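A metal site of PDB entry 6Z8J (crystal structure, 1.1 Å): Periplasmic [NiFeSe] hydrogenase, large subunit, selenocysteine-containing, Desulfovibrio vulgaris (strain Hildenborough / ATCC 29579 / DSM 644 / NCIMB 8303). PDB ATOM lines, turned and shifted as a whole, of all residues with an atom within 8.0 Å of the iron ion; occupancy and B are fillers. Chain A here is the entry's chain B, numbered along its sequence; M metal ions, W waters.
A ring nitrogen (ND1) of His 484 is in hydrogen-bond range of the backbone carbonyl oxygen (O) of Cys 481 (2.7 Å). OE2 of Glu 45 lies close to OE1 of Gln 429 (3.4 Å). The side-chain hydroxyl of Thr 292 lies within hydrogen-bond range of the side-chain carboxylate of Glu 45 (2.6 Å).
Within 4 Å of the iron ion: Glu 45, Ile 430 and His 484. Along chain A the residues within 4 Å of the iron ion span positions 45 to 484.
The iron ion is bound by water W2 (2.1 Å), water W3 (2.1 Å), NE2 of His 484 (2.1 Å), OE2 of Glu 45 (2.2 Å), O of Ile 430 (2.2 Å) and water W1 (2.3 Å).
Water W2 lies within hydrogen-bond range of the side-chain carboxylate (OE1) of Glu 271 (2.6 Å), the side-chain amide oxygen (OE1) of Gln 429 (2.7 Å) and the side-chain amino group (NZ) of Lys 306 (3.1 Å). Water W1 lies within hydrogen-bond range of the side-chain carboxylate (OE1) of Glu 45 and the side-chain amino group (NZ) of Lys 306.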
ATOM      1  N   TYR A  41      19.530 -30.204  15.620  1.00  0.00           N
ATOM      2  CA  TYR A  41      18.340 -29.369  15.639  1.00  0.00           C
ATOM      3  C   TYR A  41      18.697 -27.924  15.956  1.00  0.00           C
ATOM      4  O   TYR A  41      19.547 -27.647  16.792  1.00  0.00           O
ATOM      5  CB  TYR A  41      17.392 -29.908  16.721  1.00  0.00           C
ATOM      6  CG  TYR A  41      16.168 -29.071  17.003  1.00  0.00           C
ATOM      7  CD1 TYR A  41      15.014 -29.187  16.230  1.00  0.00           C
ATOM      8  CD2 TYR A  41      16.145 -28.164  18.058  1.00  0.00           C
ATOM      9  CE1 TYR A  41      13.874 -28.441  16.509  1.00  0.00           C
ATOM     10  CE2 TYR A  41      15.023 -27.404  18.345  1.00  0.00           C
ATOM     11  CZ  TYR A  41      13.881 -27.538  17.575  1.00  0.00           C
ATOM     12  OH  TYR A  41      12.762 -26.799  17.855  1.00  0.00           O
ATOM     13  N   GLU A  45      11.392 -22.807  13.581  1.00  0.00           N
ATOM     14  CA  GLU A  45       9.969 -22.514  13.749  1.00  0.00           C
ATOM     15  C   GLU A  45       9.701 -21.765  15.036  1.00  0.00           C
ATOM     16  O   GLU A  45       8.735 -21.002  15.099  1.00  0.00           O
ATOM     17  CB  GLU A  45       9.161 -23.803  13.636  1.00  0.00           C
ATOM     18  CG  GLU A  45       9.188 -24.376  12.215  1.00  0.00           C
ATOM     19  CD  GLU A  45       9.026 -25.872  12.141  1.00  0.00           C
ATOM     20  OE1 GLU A  45       9.332 -26.571  13.132  1.00  0.00           O
ATOM     21  OE2 GLU A  45       8.627 -26.375  11.053  1.00  0.00           O
ATOM     22  N   ILE A  63      18.146 -22.176   7.005  1.00  0.00           N
ATOM     23  CA  ILE A  63      17.877 -23.585   7.210  1.00  0.00           C
ATOM     24  C   ILE A  63      18.898 -24.425   6.449  1.00  0.00           C
ATOM     25  O   ILE A  63      19.324 -25.491   6.908  1.00  0.00           O
ATOM     26  CB  ILE A  63      16.440 -23.924   6.791  1.00  0.00           C
ATOM     27  CG1 ILE A  63      15.474 -23.289   7.792  1.00  0.00           C
ATOM     28  CG2 ILE A  63      16.258 -25.432   6.668  1.00  0.00           C
ATOM     29  CD1 ILE A  63      14.065 -23.321   7.399  1.00  0.00           C
ATOM     30  N   GLU A 271       1.967 -34.315  10.448  1.00  0.00           N
ATOM     31  CA  GLU A 271       3.304 -34.617  10.922  1.00  0.00           C
ATOM     32  C   GLU A 271       3.221 -35.364  12.247  1.00  0.00           C
ATOM     33  O   GLU A 271       2.677 -34.855  13.231  1.00  0.00           O
ATOM     34  CB  GLU A 271       4.158 -33.355  11.071  1.00  0.00           C
ATOM     35  CG  GLU A 271       4.481 -32.728   9.738  1.00  0.00           C
ATOM     36  CD  GLU A 271       5.498 -31.621   9.864  1.00  0.00           C
ATOM     37  OE1 GLU A 271       5.112 -30.483  10.226  1.00  0.00           O
ATOM     38  OE2 GLU A 271       6.682 -31.880   9.629  1.00  0.00           O
ATOM     39  N   PHE A 278      10.228 -34.747  19.913  1.00  0.00           N
ATOM     40  CA  PHE A 278       9.291 -33.663  20.141  1.00  0.00           C
ATOM     41  C   PHE A 278       8.211 -34.154  21.082  1.00  0.00           C
ATOM     42  O   PHE A 278       7.951 -35.351  21.207  1.00  0.00           O
ATOM     43  CB  PHE A 278       8.662 -33.164  18.819  1.00  0.00           C
ATOM     44  CG  PHE A 278       9.685 -32.629  17.881  1.00  0.00           C
ATOM     45  CD1 PHE A 278      10.205 -31.360  18.058  1.00  0.00           C
ATOM     46  CD2 PHE A 278      10.211 -33.438  16.900  1.00  0.00           C
ATOM     47  CE1 PHE A 278      11.191 -30.897  17.264  1.00  0.00           C
ATOM     48  CE2 PHE A 278      11.216 -32.968  16.075  1.00  0.00           C
ATOM     49  CZ  PHE A 278      11.716 -31.702  16.253  1.00  0.00           C
ATOM     50  N   TYR A 287       0.143 -28.852   9.098  1.00  0.00           N
ATOM     51  CA  TYR A 287       1.068 -27.732   9.252  1.00  0.00           C
ATOM     52  C   TYR A 287       0.369 -26.445   9.668  1.00  0.00           C
ATOM     53  O   TYR A 287       0.981 -25.600  10.318  1.00  0.00           O
ATOM     54  CB  TYR A 287       1.866 -27.522   7.955  1.00  0.00           C
ATOM     55  CG  TYR A 287       0.976 -27.293   6.774  1.00  0.00           C
ATOM     56  CD1 TYR A 287       0.524 -26.019   6.460  1.00  0.00           C
ATOM     57  CD2 TYR A 287       0.561 -28.342   5.967  1.00  0.00           C
ATOM     58  CE1 TYR A 287      -0.330 -25.805   5.393  1.00  0.00           C
ATOM     59  CE2 TYR A 287      -0.282 -28.138   4.892  1.00  0.00           C
ATOM     60  CZ  TYR A 287      -0.724 -26.860   4.598  1.00  0.00           C
ATOM     61  OH  TYR A 287      -1.599 -26.648   3.532  1.00  0.00           O
ATOM     62  N   GLY A 290       0.619 -26.608  13.204  1.00  0.00           N
ATOM     63  CA  GLY A 290       1.861 -27.244  13.616  1.00  0.00           C
ATOM     64  C   GLY A 290       2.442 -26.641  14.880  1.00  0.00           C
ATOM     65  O   GLY A 290       2.231 -25.465  15.195  1.00  0.00           O
ATOM     66  N   LYS A 291       3.202 -27.456  15.599  1.00  0.00           N
ATOM     67  CA  LYS A 291       3.852 -27.053  16.838  1.00  0.00           C
ATOM     68  C   LYS A 291       5.202 -27.726  16.901  1.00  0.00           C
ATOM     69  O   LYS A 291       5.364 -28.863  16.447  1.00  0.00           O
ATOM     70  CB  LYS A 291       3.049 -27.450  18.077  1.00  0.00           C
ATOM     71  CG  LYS A 291       1.728 -26.744  18.170  1.00  0.00           C
ATOM     72  CD  LYS A 291       1.074 -26.890  19.537  1.00  0.00           C
ATOM     73  CE  LYS A 291      -0.288 -26.200  19.521  1.00  0.00           C
ATOM     74  NZ  LYS A 291      -1.432 -27.132  19.780  1.00  0.00           N
ATOM     75  N   THR A 292       6.176 -27.020  17.456  1.00  0.00           N
ATOM     76  CA  THR A 292       7.543 -27.524  17.530  1.00  0.00           C
ATOM     77  C   THR A 292       8.024 -27.327  18.959  1.00  0.00           C
ATOM     78  O   THR A 292       8.444 -26.239  19.351  1.00  0.00           O
ATOM     79  CB  THR A 292       8.384 -26.796  16.505  1.00  0.00           C
ATOM     80  OG1 THR A 292       7.771 -26.965  15.223  1.00  0.00           O
ATOM     81  CG2 THR A 292       9.798 -27.368  16.449  1.00  0.00           C
ATOM     82  N   PHE A 304      15.491 -35.966  15.103  1.00  0.00           N
ATOM     83  CA  PHE A 304      14.888 -34.640  15.145  1.00  0.00           C
ATOM     84  C   PHE A 304      14.045 -34.320  13.917  1.00  0.00           C
ATOM     85  O   PHE A 304      13.471 -33.221  13.818  1.00  0.00           O
ATOM     86  CB  PHE A 304      15.960 -33.556  15.327  1.00  0.00           C
ATOM     87  CG  PHE A 304      16.562 -33.505  16.701  1.00  0.00           C
ATOM     88  CD1 PHE A 304      15.806 -33.123  17.778  1.00  0.00           C
ATOM     89  CD2 PHE A 304      17.901 -33.798  16.889  1.00  0.00           C
ATOM     90  CE1 PHE A 304      16.364 -33.068  19.040  1.00  0.00           C
ATOM     91  CE2 PHE A 304      18.479 -33.744  18.130  1.00  0.00           C
ATOM     92  CZ  PHE A 304      17.706 -33.382  19.221  1.00  0.00           C
ATOM     93  N   VAL A 305      13.915 -35.269  12.981  1.00  0.00           N
ATOM     94  CA  VAL A 305      13.035 -35.106  11.822  1.00  0.00           C
ATOM     95  C   VAL A 305      11.649 -35.583  12.241  1.00  0.00           C
ATOM     96  O   VAL A 305      11.526 -36.683  12.786  1.00  0.00           O
ATOM     97  CB  VAL A 305      13.569 -35.932  10.631  1.00  0.00           C
ATOM     98  CG1 VAL A 305      12.743 -35.661   9.401  1.00  0.00           C
ATOM     99  CG2 VAL A 305      15.041 -35.673  10.353  1.00  0.00           C
ATOM    100  N   LYS A 306      10.618 -34.767  12.030  1.00  0.00           N
ATOM    101  CA  LYS A 306       9.242 -35.227  12.192  1.00  0.00           C
ATOM    102  C   LYS A 306       8.914 -36.227  11.082  1.00  0.00           C
ATOM    103  O   LYS A 306       9.686 -36.418  10.143  1.00  0.00           O
ATOM    104  CB  LYS A 306       8.255 -34.055  12.151  1.00  0.00           C
ATOM    105  CG  LYS A 306       8.437 -33.012  13.283  1.00  0.00           C
ATOM    106  CD  LYS A 306       7.405 -31.890  13.169  1.00  0.00           C
ATOM    107  CE  LYS A 306       7.497 -30.861  14.293  1.00  0.00           C
ATOM    108  NZ  LYS A 306       6.735 -29.626  13.905  1.00  0.00           N
ATOM    109  N   LEU A 415       6.850 -26.696   1.625  1.00  0.00           N
ATOM    110  CA  LEU A 415       5.846 -25.698   1.940  1.00  0.00           C
ATOM    111  C   LEU A 415       6.255 -24.957   3.199  1.00  0.00           C
ATOM    112  O   LEU A 415       6.882 -25.512   4.104  1.00  0.00           O
ATOM    113  CB  LEU A 415       4.448 -26.293   2.056  1.00  0.00           C
ATOM    114  CG  LEU A 415       4.142 -27.120   3.293  1.00  0.00           C
ATOM    115  CD1 LEU A 415       3.676 -26.275   4.480  1.00  0.00           C
ATOM    116  CD2 LEU A 415       3.119 -28.217   3.002  1.00  0.00           C
ATOM    117  N   TYR A 428       5.060 -20.274  12.419  1.00  0.00           N
ATOM    118  CA  TYR A 428       5.685 -20.478  11.126  1.00  0.00           C
ATOM    119  C   TYR A 428       6.046 -21.950  11.099  1.00  0.00           C
ATOM    120  O   TYR A 428       6.742 -22.424  11.999  1.00  0.00           O
ATOM    121  CB  TYR A 428       6.931 -19.606  10.960  1.00  0.00           C
ATOM    122  CG  TYR A 428       7.338 -19.377   9.516  1.00  0.00           C
ATOM    123  CD1 TYR A 428       7.960 -20.386   8.776  1.00  0.00           C
ATOM    124  CD2 TYR A 428       7.128 -18.153   8.908  1.00  0.00           C
ATOM    125  CE1 TYR A 428       8.340 -20.159   7.455  1.00  0.00           C
ATOM    126  CE2 TYR A 428       7.507 -17.913   7.604  1.00  0.00           C
ATOM    127  CZ  TYR A 428       8.108 -18.914   6.862  1.00  0.00           C
ATOM    128  OH  TYR A 428       8.496 -18.673   5.559  1.00  0.00           O
ATOM    129  N   GLN A 429       5.560 -22.674  10.111  1.00  0.00           N
ATOM    130  CA  GLN A 429       5.773 -24.106  10.026  1.00  0.00           C
ATOM    131  C   GLN A 429       6.335 -24.456   8.657  1.00  0.00           C
ATOM    132  O   GLN A 429       5.856 -23.965   7.622  1.00  0.00           O
ATOM    133  CB  GLN A 429       4.491 -24.920  10.313  1.00  0.00           C
ATOM    134  CG  GLN A 429       4.102 -24.846  11.773  1.00  0.00           C
ATOM    135  CD  GLN A 429       5.052 -25.621  12.667  1.00  0.00           C
ATOM    136  OE1 GLN A 429       5.492 -26.707  12.327  1.00  0.00           O
ATOM    137  NE2 GLN A 429       5.346 -25.079  13.830  1.00  0.00           N
ATOM    138  N   ILE A 430       7.347 -25.311   8.672  1.00  0.00           N
ATOM    139  CA  ILE A 430       8.072 -25.710   7.475  1.00  0.00           C
ATOM    140  C   ILE A 430       7.952 -27.222   7.333  1.00  0.00           C
ATOM    141  O   ILE A 430       8.213 -27.978   8.273  1.00  0.00           O
ATOM    142  CB  ILE A 430       9.548 -25.273   7.551  1.00  0.00           C
ATOM    143  CG1 ILE A 430       9.601 -23.738   7.537  1.00  0.00           C
ATOM    144  CG2 ILE A 430      10.351 -25.857   6.399  1.00  0.00           C
ATOM    145  CD1 ILE A 430      10.704 -23.187   8.374  1.00  0.00           C
ATOM    146  N   VAL A 431       7.579 -27.649   6.129  1.00  0.00           N
ATOM    147  CA  VAL A 431       7.510 -29.064   5.745  1.00  0.00           C
ATOM    148  C   VAL A 431       8.345 -29.184   4.468  1.00  0.00           C
ATOM    149  O   VAL A 431       7.903 -28.744   3.401  1.00  0.00           O
ATOM    150  CB  VAL A 431       6.052 -29.504   5.528  1.00  0.00           C
ATOM    151  CG1 VAL A 431       5.937 -30.957   5.141  1.00  0.00           C
ATOM    152  CG2 VAL A 431       5.234 -29.229   6.797  1.00  0.00           C
ATOM    153  N   SER A 432       9.542 -29.769   4.576  1.00  0.00           N
ATOM    154  CA  SER A 432      10.575 -29.671   3.544  1.00  0.00           C
ATOM    155  C   SER A 432      10.812 -31.024   2.855  1.00  0.00           C
ATOM    156  O   SER A 432      10.251 -32.054   3.234  1.00  0.00           O
ATOM    157  CB  SER A 432      11.878 -29.210   4.174  1.00  0.00           C
ATOM    158  OG  SER A 432      12.255 -30.209   5.098  1.00  0.00           O
ATOM    159  N   LEU A 435      12.648 -33.798   4.754  1.00  0.00           N
ATOM    160  CA  LEU A 435      11.707 -34.257   5.760  1.00  0.00           C
ATOM    161  C   LEU A 435      10.855 -35.387   5.202  1.00  0.00           C
ATOM    162  O   LEU A 435      10.718 -36.443   5.830  1.00  0.00           O
ATOM    163  CB  LEU A 435      10.841 -33.073   6.194  1.00  0.00           C
ATOM    164  CG  LEU A 435       9.574 -33.407   6.964  1.00  0.00           C
ATOM    165  CD1 LEU A 435       9.849 -33.816   8.390  1.00  0.00           C
ATOM    166  CD2 LEU A 435       8.644 -32.205   6.927  1.00  0.00           C
ATOM    167  N   CYS A 481      17.646 -29.028   6.042  1.00  0.00           N
ATOM    168  CA  CYS A 481      16.252 -28.887   5.628  1.00  0.00           C
ATOM    169  C   CYS A 481      15.321 -29.806   6.413  1.00  0.00           C
ATOM    170  O   CYS A 481      14.212 -29.410   6.776  1.00  0.00           O
ATOM    171  CB  CYS A 481      16.128 -29.255   4.160  1.00  0.00           C
ATOM    172  SG  CYS A 481      16.534 -27.902   3.021  1.00  0.00           S
ATOM    173  N   ALA A 482      15.717 -31.057   6.610  1.00  0.00           N
ATOM    174  CA  ALA A 482      14.797 -32.024   7.180  1.00  0.00           C
ATOM    175  C   ALA A 482      14.375 -31.656   8.586  1.00  0.00           C
ATOM    176  O   ALA A 482      13.211 -31.864   8.947  1.00  0.00           O
ATOM    177  CB  ALA A 482      15.412 -33.429   7.142  1.00  0.00           C
ATOM    178  N   VAL A 483      15.290 -31.137   9.398  1.00  0.00           N
ATOM    179  CA  VAL A 483      15.045 -30.815  10.803  1.00  0.00           C
ATOM    180  C   VAL A 483      14.690 -29.352  11.004  1.00  0.00           C
ATOM    181  O   VAL A 483      13.804 -29.030  11.798  1.00  0.00           O
ATOM    182  CB  VAL A 483      16.271 -31.187  11.666  1.00  0.00           C
ATOM    183  CG1 VAL A 483      15.997 -30.792  13.098  1.00  0.00           C
ATOM    184  CG2 VAL A 483      16.618 -32.647  11.545  1.00  0.00           C
ATOM    185  N   HIS A 484      15.437 -28.466  10.357  1.00  0.00           N
ATOM    186  CA  HIS A 484      15.286 -27.022  10.573  1.00  0.00           C
ATOM    187  C   HIS A 484      15.218 -26.649  12.060  1.00  0.00           C
ATOM    188  O   HIS A 484      16.065 -27.142  12.842  1.00  0.00           O
ATOM    189  CB  HIS A 484      14.153 -26.380   9.712  1.00  0.00           C
ATOM    190  CG  HIS A 484      12.881 -27.177   9.631  1.00  0.00           C
ATOM    191  ND1 HIS A 484      12.743 -28.264   8.791  1.00  0.00           N
ATOM    192  CD2 HIS A 484      11.697 -27.058  10.288  1.00  0.00           C
ATOM    193  CE1 HIS A 484      11.524 -28.759   8.919  1.00  0.00           C
ATOM    194  NE2 HIS A 484      10.881 -28.071   9.840  1.00  0.00           N
ATOM    195  OXT HIS A 484      14.363 -25.826  12.478  1.00  0.00           O
HETATM  196 FE    FE M   1       8.832 -28.424  10.347  1.00  0.00          FE
HETATM  197  O   HOH W   1       9.430 -29.077  12.429  1.00  0.00           O
HETATM  198  O   HOH W   2       6.807 -28.639  10.972  1.00  0.00           O
HETATM  199  O   HOH W   3       8.918 -30.472   9.744  1.00  0.00           O
